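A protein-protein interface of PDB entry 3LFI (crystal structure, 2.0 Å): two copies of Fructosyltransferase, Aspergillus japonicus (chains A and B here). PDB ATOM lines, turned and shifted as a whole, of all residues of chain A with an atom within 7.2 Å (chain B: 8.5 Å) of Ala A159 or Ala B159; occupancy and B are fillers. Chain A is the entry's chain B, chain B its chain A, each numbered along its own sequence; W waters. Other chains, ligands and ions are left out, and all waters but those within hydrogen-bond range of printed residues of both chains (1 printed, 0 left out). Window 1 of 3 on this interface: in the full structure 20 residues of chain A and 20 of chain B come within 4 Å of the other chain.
The backbone NH of Gly A155 lies within hydrogen-bond range of the backbone carbonyl oxygen of Arg B132, at 2.8 Å. The guanidinium group (NH2) of Arg B132 lies within hydrogen-bond range of the backbone carbonyl oxygen (O) of Val A157, 3.2 Å away. The backbone NH (N) of Gly B155 lies within hydrogen-bond range of the backbone carbonyl oxygen (O) of Arg A132 (2.8 Å). The guanidinium group (NH2) of Arg A132 lies within hydrogen-bond range of the backbone carbonyl oxygen (O) of Val B157, 3.1 Å away. The side-chain amide oxygen (OE1) of Gln B241 sits at hydrogen-bond distance from the guanidinium group (NH1) of Arg A132 (2.7 Å).
Among the printed residues, merely in contact across the chains: Ala A159 with Ala B159 (3.6 Å), Arg A132 with Pro B156 (3.9 Å) and Pro A156 with Arg B132 (3.98 Å).
Of the 14 printed residues of chain A, 5 touch a printed residue of chain B. Of the 21 printed residues of chain B, 6 touch a printed residue of chain A. Hydrophobic or aromatic side chains of chain B that line the printed part of chain A: Ala B159. Among the printed residues, 8 pairs touch across the chains.
The side-chain carboxylate (OD1) of Asp B160 is in salt-bridge range of the guanidinium group (NE) of Arg B132 (3.0 Å). O of Gln B137 lies within hydrogen-bond range of N of Val B157, 2.8 Å away. The guanidinium group of Arg A132 lies within salt-bridge range of the side-chain carboxylate of Asp A160. O of Gln A137 lies within hydrogen-bond range of N of Val A157 (2.8 Å).
Water W1 lies within hydrogen-bond range of O of Val B157 (2.7 Å), N of Trp B243 (2.8 Å) and NH2 of Arg A132 (3.4 Å).
Arg A132 touches Gly B155, and with the chains exchanged Gly A155 touches Arg B132. Arg A132 touches Pro B156, and with the chains exchanged Pro A156 touches Arg B132. Arg A132 touches Val B157, and with the chains exchanged Val A157 touches Arg B132. Ala B159 touches its own counterpart, Ala A159. Positions printed for both chains: 132, 133, 135, 136, 137, 138, 155, 156, 157, 158, 159, 160, 161 and 170. Of the 8 pairs that touch across the chains among the printed residues, 7 have their exchanged pair printed and touching as well.
Gly A133 touches none of the printed residues of chain B. Ile A158 touches none of the printed residues of chain B. Ala A159 touches just one residue of chain B: Ala B159. Of the printed residues of chain A, Gly B155 touches Arg A132. Printed residues of chain A within 4 Å of Val B157: Arg A132 (3.1 Å). Of chain A, only Ala A159 comes within 4 Å of Ala B159. The nearest residue of chain A that does not touch Ala B159 is Asp A160 (4.3 Å). The nearest printed residue of chain A that does not touch Gln B241 is Gly A133 (6.4 Å).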
ATOM      1  N   ARG A 132     -20.502   2.660  -6.819  1.00  0.00           N
ATOM      2  CA  ARG A 132     -20.914   2.345  -5.453  1.00  0.00           C
ATOM      3  C   ARG A 132     -21.143   0.838  -5.307  1.00  0.00           C
ATOM      4  O   ARG A 132     -21.749   0.212  -6.174  1.00  0.00           O
ATOM      5  CB  ARG A 132     -22.202   3.119  -5.106  1.00  0.00           C
ATOM      6  CG  ARG A 132     -22.689   3.006  -3.643  1.00  0.00           C
ATOM      7  CD  ARG A 132     -21.871   3.893  -2.685  1.00  0.00           C
ATOM      8  NE  ARG A 132     -22.433   3.956  -1.330  1.00  0.00           N
ATOM      9  CZ  ARG A 132     -23.574   4.563  -1.003  1.00  0.00           C
ATOM     10  NH1 ARG A 132     -24.308   5.178  -1.921  1.00  0.00           N
ATOM     11  NH2 ARG A 132     -23.989   4.560   0.253  1.00  0.00           N
ATOM     12  N   GLY A 133     -20.641   0.266  -4.215  1.00  0.00           N
ATOM     13  CA  GLY A 133     -20.812  -1.150  -3.959  1.00  0.00           C
ATOM     14  C   GLY A 133     -19.836  -2.042  -4.699  1.00  0.00           C
ATOM     15  O   GLY A 133     -19.950  -3.263  -4.640  1.00  0.00           O
ATOM     16  N   GLU A 135     -16.577  -2.674  -4.169  1.00  0.00           N
ATOM     17  CA  GLU A 135     -15.789  -3.476  -3.248  1.00  0.00           C
ATOM     18  C   GLU A 135     -16.319  -3.433  -1.821  1.00  0.00           C
ATOM     19  O   GLU A 135     -16.520  -2.351  -1.259  1.00  0.00           O
ATOM     20  CB  GLU A 135     -14.343  -2.965  -3.245  1.00  0.00           C
ATOM     21  CG  GLU A 135     -13.701  -2.875  -4.622  1.00  0.00           C
ATOM     22  CD  GLU A 135     -12.482  -1.969  -4.639  1.00  0.00           C
ATOM     23  OE1 GLU A 135     -12.623  -0.770  -4.319  1.00  0.00           O
ATOM     24  OE2 GLU A 135     -11.388  -2.453  -4.977  1.00  0.00           O
ATOM     25  N   THR A 136     -16.539  -4.609  -1.241  1.00  0.00           N
ATOM     26  CA  THR A 136     -17.002  -4.719   0.138  1.00  0.00           C
ATOM     27  C   THR A 136     -16.096  -5.734   0.820  1.00  0.00           C
ATOM     28  O   THR A 136     -15.388  -6.486   0.146  1.00  0.00           O
ATOM     29  CB  THR A 136     -18.474  -5.200   0.236  1.00  0.00           C
ATOM     30  OG1 THR A 136     -18.608  -6.515  -0.331  1.00  0.00           O
ATOM     31  CG2 THR A 136     -19.399  -4.218  -0.501  1.00  0.00           C
ATOM     32  N   GLN A 137     -16.111  -5.763   2.147  1.00  0.00           N
ATOM     33  CA  GLN A 137     -15.263  -6.703   2.865  1.00  0.00           C
ATOM     34  C   GLN A 137     -16.136  -7.788   3.506  1.00  0.00           C
ATOM     35  O   GLN A 137     -17.006  -7.495   4.334  1.00  0.00           O
ATOM     36  CB  GLN A 137     -14.436  -5.956   3.921  1.00  0.00           C
ATOM     37  CG  GLN A 137     -13.946  -4.570   3.469  1.00  0.00           C
ATOM     38  CD  GLN A 137     -13.196  -4.586   2.147  1.00  0.00           C
ATOM     39  OE1 GLN A 137     -13.209  -3.596   1.411  1.00  0.00           O
ATOM     40  NE2 GLN A 137     -12.532  -5.696   1.843  1.00  0.00           N
ATOM     41  N   SER A 138     -15.911  -9.036   3.110  1.00  0.00           N
ATOM     42  CA  SER A 138     -16.702 -10.153   3.619  1.00  0.00           C
ATOM     43  C   SER A 138     -15.863 -11.173   4.376  1.00  0.00           C
ATOM     44  O   SER A 138     -14.635 -11.151   4.308  1.00  0.00           O
ATOM     45  CB  SER A 138     -17.434 -10.843   2.458  1.00  0.00           C
ATOM     46  OG  SER A 138     -18.302  -9.933   1.800  1.00  0.00           O
ATOM     47  N   GLY A 155     -24.306 -11.050   4.345  1.00  0.00           N
ATOM     48  CA  GLY A 155     -23.682  -9.973   3.589  1.00  0.00           C
ATOM     49  C   GLY A 155     -22.318  -9.586   4.117  1.00  0.00           C
ATOM     50  O   GLY A 155     -21.868 -10.138   5.123  1.00  0.00           O
ATOM     51  N   PRO A 156     -21.626  -8.643   3.458  1.00  0.00           N
ATOM     52  CA  PRO A 156     -20.295  -8.201   3.898  1.00  0.00           C
ATOM     53  C   PRO A 156     -20.338  -7.594   5.303  1.00  0.00           C
ATOM     54  O   PRO A 156     -21.355  -7.026   5.682  1.00  0.00           O
ATOM     55  CB  PRO A 156     -19.896  -7.172   2.832  1.00  0.00           C
ATOM     56  CG  PRO A 156     -21.230  -6.652   2.315  1.00  0.00           C
ATOM     57  CD  PRO A 156     -22.065  -7.916   2.251  1.00  0.00           C
ATOM     58  N   VAL A 157     -19.250  -7.717   6.070  1.00  0.00           N
ATOM     59  CA  VAL A 157     -19.213  -7.146   7.426  1.00  0.00           C
ATOM     60  C   VAL A 157     -18.864  -5.666   7.412  1.00  0.00           C
ATOM     61  O   VAL A 157     -19.003  -4.973   8.417  1.00  0.00           O
ATOM     62  CB  VAL A 157     -18.226  -7.887   8.358  1.00  0.00           C
ATOM     63  CG1 VAL A 157     -18.730  -9.291   8.611  1.00  0.00           C
ATOM     64  CG2 VAL A 157     -16.837  -7.911   7.758  1.00  0.00           C
ATOM     65  N   ILE A 158     -18.374  -5.206   6.268  1.00  0.00           N
ATOM     66  CA  ILE A 158     -18.066  -3.803   6.023  1.00  0.00           C
ATOM     67  C   ILE A 158     -18.673  -3.670   4.629  1.00  0.00           C
ATOM     68  O   ILE A 158     -18.004  -3.880   3.621  1.00  0.00           O
ATOM     69  CB  ILE A 158     -16.544  -3.525   6.008  1.00  0.00           C
ATOM     70  CG1 ILE A 158     -15.980  -3.651   7.432  1.00  0.00           C
ATOM     71  CG2 ILE A 158     -16.275  -2.110   5.485  1.00  0.00           C
ATOM     72  CD1 ILE A 158     -14.472  -3.343   7.544  1.00  0.00           C
ATOM     73  N   ALA A 159     -19.966  -3.348   4.593  1.00  0.00           N
ATOM     74  CA  ALA A 159     -20.713  -3.266   3.334  1.00  0.00           C
ATOM     75  C   ALA A 159     -20.606  -1.986   2.516  1.00  0.00           C
ATOM     76  O   ALA A 159     -21.275  -1.843   1.497  1.00  0.00           O
ATOM     77  CB  ALA A 159     -22.185  -3.575   3.608  1.00  0.00           C
ATOM     78  N   ASP A 160     -19.768  -1.054   2.942  1.00  0.00           N
ATOM     79  CA  ASP A 160     -19.644   0.185   2.194  1.00  0.00           C
ATOM     80  C   ASP A 160     -18.417   0.950   2.659  1.00  0.00           C
ATOM     81  O   ASP A 160     -17.949   0.762   3.782  1.00  0.00           O
ATOM     82  CB  ASP A 160     -20.916   1.019   2.400  1.00  0.00           C
ATOM     83  CG  ASP A 160     -20.994   2.225   1.478  1.00  0.00           C
ATOM     84  OD1 ASP A 160     -20.391   2.200   0.380  1.00  0.00           O
ATOM     85  OD2 ASP A 160     -21.685   3.196   1.855  1.00  0.00           O
ATOM     86  N   HIS A 161     -17.882   1.791   1.781  1.00  0.00           N
ATOM     87  CA  HIS A 161     -16.723   2.595   2.123  1.00  0.00           C
ATOM     88  C   HIS A 161     -17.233   3.728   3.015  1.00  0.00           C
ATOM     89  O   HIS A 161     -18.445   3.902   3.167  1.00  0.00           O
ATOM     90  CB  HIS A 161     -16.088   3.157   0.849  1.00  0.00           C
ATOM     91  CG  HIS A 161     -17.029   3.977   0.020  1.00  0.00           C
ATOM     92  ND1 HIS A 161     -17.520   5.198   0.436  1.00  0.00           N
ATOM     93  CD2 HIS A 161     -17.592   3.736  -1.186  1.00  0.00           C
ATOM     94  CE1 HIS A 161     -18.346   5.672  -0.480  1.00  0.00           C
ATOM     95  NE2 HIS A 161     -18.409   4.803  -1.474  1.00  0.00           N
ATOM     96  N   PHE A 170     -11.217   0.705  -2.424  1.00  0.00           N
ATOM     97  CA  PHE A 170     -11.519   0.342  -1.046  1.00  0.00           C
ATOM     98  C   PHE A 170     -11.336  -1.166  -0.952  1.00  0.00           C
ATOM     99  O   PHE A 170     -12.303  -1.917  -0.849  1.00  0.00           O
ATOM    100  CB  PHE A 170     -12.964   0.737  -0.724  1.00  0.00           C
ATOM    101  CG  PHE A 170     -13.354   0.534   0.717  1.00  0.00           C
ATOM    102  CD1 PHE A 170     -12.739   1.261   1.733  1.00  0.00           C
ATOM    103  CD2 PHE A 170     -14.370  -0.353   1.053  1.00  0.00           C
ATOM    104  CE1 PHE A 170     -13.132   1.113   3.064  1.00  0.00           C
ATOM    105  CE2 PHE A 170     -14.773  -0.511   2.386  1.00  0.00           C
ATOM    106  CZ  PHE A 170     -14.150   0.228   3.393  1.00  0.00           C
ATOM    107  N   ASN B  93     -27.937  -6.890  -6.333  1.00  0.00           N
ATOM    108  CA  ASN B  93     -28.372  -6.321  -5.052  1.00  0.00           C
ATOM    109  C   ASN B  93     -29.582  -7.055  -4.449  1.00  0.00           C
ATOM    110  O   ASN B  93     -29.760  -7.064  -3.224  1.00  0.00           O
ATOM    111  CB  ASN B  93     -28.752  -4.844  -5.221  1.00  0.00           C
ATOM    112  CG  ASN B  93     -27.645  -4.022  -5.835  1.00  0.00           C
ATOM    113  OD1 ASN B  93     -26.486  -4.420  -5.816  1.00  0.00           O
ATOM    114  ND2 ASN B  93     -27.999  -2.860  -6.378  1.00  0.00           N
ATOM    115  N   SER B 118     -33.994  -4.270  -1.548  1.00  0.00           N
ATOM    116  CA  SER B 118     -33.482  -5.377  -2.332  1.00  0.00           C
ATOM    117  C   SER B 118     -33.083  -6.422  -1.300  1.00  0.00           C
ATOM    118  O   SER B 118     -32.401  -6.098  -0.324  1.00  0.00           O
ATOM    119  CB  SER B 118     -32.279  -4.911  -3.153  1.00  0.00           C
ATOM    120  OG  SER B 118     -31.590  -3.874  -2.479  1.00  0.00           O
ATOM    121  N   ARG B 132     -27.177 -10.433   8.604  1.00  0.00           N
ATOM    122  CA  ARG B 132     -26.567  -9.199   8.107  1.00  0.00           C
ATOM    123  C   ARG B 132     -26.660  -9.158   6.579  1.00  0.00           C
ATOM    124  O   ARG B 132     -26.423 -10.167   5.913  1.00  0.00           O
ATOM    125  CB  ARG B 132     -25.089  -9.128   8.550  1.00  0.00           C
ATOM    126  CG  ARG B 132     -24.341  -7.818   8.196  1.00  0.00           C
ATOM    127  CD  ARG B 132     -24.769  -6.636   9.084  1.00  0.00           C
ATOM    128  NE  ARG B 132     -23.952  -5.435   8.881  1.00  0.00           N
ATOM    129  CZ  ARG B 132     -22.670  -5.319   9.228  1.00  0.00           C
ATOM    130  NH1 ARG B 132     -22.028  -6.327   9.806  1.00  0.00           N
ATOM    131  NH2 ARG B 132     -22.018  -4.189   8.995  1.00  0.00           N
ATOM    132  N   GLY B 133     -27.017  -7.994   6.042  1.00  0.00           N
ATOM    133  CA  GLY B 133     -27.122  -7.819   4.603  1.00  0.00           C
ATOM    134  C   GLY B 133     -28.391  -8.382   3.989  1.00  0.00           C
ATOM    135  O   GLY B 133     -28.495  -8.477   2.765  1.00  0.00           O
ATOM    136  N   SER B 134     -29.343  -8.759   4.845  1.00  0.00           N
ATOM    137  CA  SER B 134     -30.623  -9.313   4.427  1.00  0.00           C
ATOM    138  C   SER B 134     -31.389  -8.357   3.535  1.00  0.00           C
ATOM    139  O   SER B 134     -31.873  -8.730   2.459  1.00  0.00           O
ATOM    140  CB  SER B 134     -31.503  -9.620   5.649  1.00  0.00           C
ATOM    141  OG  SER B 134     -31.129 -10.837   6.263  1.00  0.00           O
ATOM    142  N   GLU B 135     -31.501  -7.123   4.007  1.00  0.00           N
ATOM    143  CA  GLU B 135     -32.243  -6.090   3.310  1.00  0.00           C
ATOM    144  C   GLU B 135     -31.413  -4.827   3.148  1.00  0.00           C
ATOM    145  O   GLU B 135     -30.839  -4.332   4.121  1.00  0.00           O
ATOM    146  CB  GLU B 135     -33.502  -5.746   4.113  1.00  0.00           C
ATOM    147  CG  GLU B 135     -34.326  -6.952   4.518  1.00  0.00           C
ATOM    148  CD  GLU B 135     -35.325  -6.638   5.615  1.00  0.00           C
ATOM    149  OE1 GLU B 135     -34.896  -6.224   6.719  1.00  0.00           O
ATOM    150  OE2 GLU B 135     -36.534  -6.816   5.374  1.00  0.00           O
ATOM    151  N   THR B 136     -31.364  -4.314   1.919  1.00  0.00           N
ATOM    152  CA  THR B 136     -30.647  -3.083   1.601  1.00  0.00           C
ATOM    153  C   THR B 136     -31.609  -2.224   0.781  1.00  0.00           C
ATOM    154  O   THR B 136     -32.677  -2.688   0.394  1.00  0.00           O
ATOM    155  CB  THR B 136     -29.342  -3.353   0.794  1.00  0.00           C
ATOM    156  OG1 THR B 136     -29.639  -4.061  -0.421  1.00  0.00           O
ATOM    157  CG2 THR B 136     -28.370  -4.183   1.632  1.00  0.00           C
ATOM    158  N   GLN B 137     -31.259  -0.971   0.529  1.00  0.00           N
ATOM    159  CA  GLN B 137     -32.154  -0.121  -0.251  1.00  0.00           C
ATOM    160  C   GLN B 137     -31.442   0.259  -1.552  1.00  0.00           C
ATOM    161  O   GLN B 137     -30.377   0.881  -1.525  1.00  0.00           O
ATOM    162  CB  GLN B 137     -32.537   1.129   0.562  1.00  0.00           C
ATOM    163  CG  GLN B 137     -32.824   0.855   2.048  1.00  0.00           C
ATOM    164  CD  GLN B 137     -33.879  -0.222   2.289  1.00  0.00           C
ATOM    165  OE1 GLN B 137     -33.824  -0.939   3.292  1.00  0.00           O
ATOM    166  NE2 GLN B 137     -34.845  -0.334   1.382  1.00  0.00           N
ATOM    167  N   SER B 138     -32.019  -0.146  -2.684  1.00  0.00           N
ATOM    168  CA  SER B 138     -31.430   0.124  -3.998  1.00  0.00           C
ATOM    169  C   SER B 138     -32.329   1.013  -4.861  1.00  0.00           C
ATOM    170  O   SER B 138     -33.519   1.183  -4.578  1.00  0.00           O
ATOM    171  CB  SER B 138     -31.162  -1.192  -4.752  1.00  0.00           C
ATOM    172  OG  SER B 138     -30.305  -2.069  -4.027  1.00  0.00           O
ATOM    173  N   GLY B 155     -24.313  -0.892  -6.500  1.00  0.00           N
ATOM    174  CA  GLY B 155     -24.856  -1.434  -5.268  1.00  0.00           C
ATOM    175  C   GLY B 155     -25.916  -0.555  -4.638  1.00  0.00           C
ATOM    176  O   GLY B 155     -26.191   0.536  -5.130  1.00  0.00           O
ATOM    177  N   PRO B 156     -26.530  -1.012  -3.537  1.00  0.00           N
ATOM    178  CA  PRO B 156     -27.570  -0.246  -2.841  1.00  0.00           C
ATOM    179  C   PRO B 156     -27.074   1.132  -2.397  1.00  0.00           C
ATOM    180  O   PRO B 156     -25.878   1.306  -2.144  1.00  0.00           O
ATOM    181  CB  PRO B 156     -27.927  -1.139  -1.653  1.00  0.00           C
ATOM    182  CG  PRO B 156     -26.639  -1.961  -1.423  1.00  0.00           C
ATOM    183  CD  PRO B 156     -26.207  -2.268  -2.830  1.00  0.00           C
ATOM    184  N   VAL B 157     -27.984   2.102  -2.306  1.00  0.00           N
ATOM    185  CA  VAL B 157     -27.609   3.452  -1.873  1.00  0.00           C
ATOM    186  C   VAL B 157     -27.596   3.540  -0.354  1.00  0.00           C
ATOM    187  O   VAL B 157     -27.054   4.478   0.222  1.00  0.00           O
ATOM    188  CB  VAL B 157     -28.553   4.544  -2.444  1.00  0.00           C
ATOM    189  CG1 VAL B 157     -28.300   4.703  -3.940  1.00  0.00           C
ATOM    190  CG2 VAL B 157     -29.993   4.187  -2.186  1.00  0.00           C
ATOM    191  N   ILE B 158     -28.231   2.565   0.283  1.00  0.00           N
ATOM    192  CA  ILE B 158     -28.247   2.456   1.735  1.00  0.00           C
ATOM    193  C   ILE B 158     -27.931   0.977   1.877  1.00  0.00           C
ATOM    194  O   ILE B 158     -28.828   0.134   1.909  1.00  0.00           O
ATOM    195  CB  ILE B 158     -29.624   2.791   2.322  1.00  0.00           C
ATOM    196  CG1 ILE B 158     -29.905   4.285   2.133  1.00  0.00           C
ATOM    197  CG2 ILE B 158     -29.659   2.443   3.809  1.00  0.00           C
ATOM    198  CD1 ILE B 158     -31.275   4.729   2.645  1.00  0.00           C
ATOM    199  N   ALA B 159     -26.636   0.680   1.936  1.00  0.00           N
ATOM    200  CA  ALA B 159     -26.144  -0.699   1.978  1.00  0.00           C
ATOM    201  C   ALA B 159     -26.170  -1.451   3.301  1.00  0.00           C
ATOM    202  O   ALA B 159     -25.793  -2.617   3.359  1.00  0.00           O
ATOM    203  CB  ALA B 159     -24.727  -0.739   1.388  1.00  0.00           C
ATOM    204  N   ASP B 160     -26.619  -0.809   4.366  1.00  0.00           N
ATOM    205  CA  ASP B 160     -26.648  -1.502   5.647  1.00  0.00           C
ATOM    206  C   ASP B 160     -27.547  -0.750   6.619  1.00  0.00           C
ATOM    207  O   ASP B 160     -27.782   0.439   6.454  1.00  0.00           O
ATOM    208  CB  ASP B 160     -25.212  -1.610   6.181  1.00  0.00           C
ATOM    209  CG  ASP B 160     -25.100  -2.457   7.446  1.00  0.00           C
ATOM    210  OD1 ASP B 160     -25.853  -3.440   7.607  1.00  0.00           O
ATOM    211  OD2 ASP B 160     -24.226  -2.140   8.279  1.00  0.00           O
ATOM    212  N   HIS B 161     -28.075  -1.455   7.614  1.00  0.00           N
ATOM    213  CA  HIS B 161     -28.926  -0.817   8.612  1.00  0.00           C
ATOM    214  C   HIS B 161     -27.987  -0.023   9.523  1.00  0.00           C
ATOM    215  O   HIS B 161     -26.766  -0.157   9.420  1.00  0.00           O
ATOM    216  CB  HIS B 161     -29.671  -1.877   9.422  1.00  0.00           C
ATOM    217  CG  HIS B 161     -28.769  -2.861  10.101  1.00  0.00           C
ATOM    218  ND1 HIS B 161     -27.849  -2.491  11.060  1.00  0.00           N
ATOM    219  CD2 HIS B 161     -28.641  -4.201   9.953  1.00  0.00           C
ATOM    220  CE1 HIS B 161     -27.194  -3.561  11.474  1.00  0.00           C
ATOM    221  NE2 HIS B 161     -27.654  -4.611  10.818  1.00  0.00           N
ATOM    222  N   PRO B 162     -28.538   0.822  10.411  1.00  0.00           N
ATOM    223  CA  PRO B 162     -27.686   1.609  11.314  1.00  0.00           C
ATOM    224  C   PRO B 162     -26.583   0.772  11.983  1.00  0.00           C
ATOM    225  O   PRO B 162     -26.835  -0.334  12.472  1.00  0.00           O
ATOM    226  CB  PRO B 162     -28.692   2.176  12.302  1.00  0.00           C
ATOM    227  CG  PRO B 162     -29.859   2.485  11.379  1.00  0.00           C
ATOM    228  CD  PRO B 162     -29.950   1.223  10.537  1.00  0.00           C
ATOM    229  N   PHE B 170     -35.515  -4.052   8.329  1.00  0.00           N
ATOM    230  CA  PHE B 170     -35.036  -2.786   7.786  1.00  0.00           C
ATOM    231  C   PHE B 170     -35.497  -2.725   6.326  1.00  0.00           C
ATOM    232  O   PHE B 170     -34.699  -2.893   5.401  1.00  0.00           O
ATOM    233  CB  PHE B 170     -33.507  -2.765   7.888  1.00  0.00           C
ATOM    234  CG  PHE B 170     -32.873  -1.472   7.463  1.00  0.00           C
ATOM    235  CD1 PHE B 170     -33.090  -0.299   8.182  1.00  0.00           C
ATOM    236  CD2 PHE B 170     -32.023  -1.435   6.360  1.00  0.00           C
ATOM    237  CE1 PHE B 170     -32.470   0.898   7.809  1.00  0.00           C
ATOM    238  CE2 PHE B 170     -31.398  -0.244   5.978  1.00  0.00           C
ATOM    239  CZ  PHE B 170     -31.624   0.927   6.709  1.00  0.00           C
ATOM    240  N   TYR B 230     -33.987   8.847   7.273  1.00  0.00           N
ATOM    241  CA  TYR B 230     -32.849   9.287   6.464  1.00  0.00           C
ATOM    242  C   TYR B 230     -33.291  10.443   5.574  1.00  0.00           C
ATOM    243  O   TYR B 230     -34.486  10.681   5.393  1.00  0.00           O
ATOM    244  CB  TYR B 230     -32.362   8.171   5.526  1.00  0.00           C
ATOM    245  CG  TYR B 230     -31.884   6.909   6.194  1.00  0.00           C
ATOM    246  CD1 TYR B 230     -30.523   6.638   6.326  1.00  0.00           C
ATOM    247  CD2 TYR B 230     -32.798   5.979   6.694  1.00  0.00           C
ATOM    248  CE1 TYR B 230     -30.083   5.465   6.946  1.00  0.00           C
ATOM    249  CE2 TYR B 230     -32.371   4.812   7.311  1.00  0.00           C
ATOM    250  CZ  TYR B 230     -31.016   4.562   7.434  1.00  0.00           C
ATOM    251  OH  TYR B 230     -30.607   3.415   8.060  1.00  0.00           O
ATOM    252  N   GLN B 241     -27.305   9.591  -4.215  1.00  0.00           N
ATOM    253  CA  GLN B 241     -26.383   8.522  -3.860  1.00  0.00           C
ATOM    254  C   GLN B 241     -26.233   8.310  -2.350  1.00  0.00           C
ATOM    255  O   GLN B 241     -26.327   7.176  -1.859  1.00  0.00           O
ATOM    256  CB  GLN B 241     -25.011   8.805  -4.474  1.00  0.00           C
ATOM    257  CG  GLN B 241     -24.010   7.682  -4.309  1.00  0.00           C
ATOM    258  CD  GLN B 241     -24.360   6.455  -5.134  1.00  0.00           C
ATOM    259  OE1 GLN B 241     -24.536   5.368  -4.593  1.00  0.00           O
ATOM    260  NE2 GLN B 241     -24.457   6.629  -6.452  1.00  0.00           N
ATOM    261  N   TRP B 243     -27.436   9.055   1.630  1.00  0.00           N
ATOM    262  CA  TRP B 243     -28.545   9.451   2.494  1.00  0.00           C
ATOM    263  C   TRP B 243     -28.104   9.471   3.953  1.00  0.00           C
ATOM    264  O   TRP B 243     -27.795   8.430   4.522  1.00  0.00           O
ATOM    265  CB  TRP B 243     -29.717   8.482   2.300  1.00  0.00           C
ATOM    266  CG  TRP B 243     -30.121   8.377   0.862  1.00  0.00           C
ATOM    267  CD1 TRP B 243     -29.425   7.761  -0.150  1.00  0.00           C
ATOM    268  CD2 TRP B 243     -31.262   8.983   0.248  1.00  0.00           C
ATOM    269  NE1 TRP B 243     -30.066   7.954  -1.351  1.00  0.00           N
ATOM    270  CE2 TRP B 243     -31.195   8.700  -1.136  1.00  0.00           C
ATOM    271  CE3 TRP B 243     -32.338   9.741   0.731  1.00  0.00           C
ATOM    272  CZ2 TRP B 243     -32.163   9.151  -2.040  1.00  0.00           C
ATOM    273  CZ3 TRP B 243     -33.300  10.186  -0.168  1.00  0.00           C
ATOM    274  CH2 TRP B 243     -33.202   9.890  -1.537  1.00  0.00           C
HETATM  275  O   HOH W   1     -26.286   6.476   1.897  1.00  0.00           O
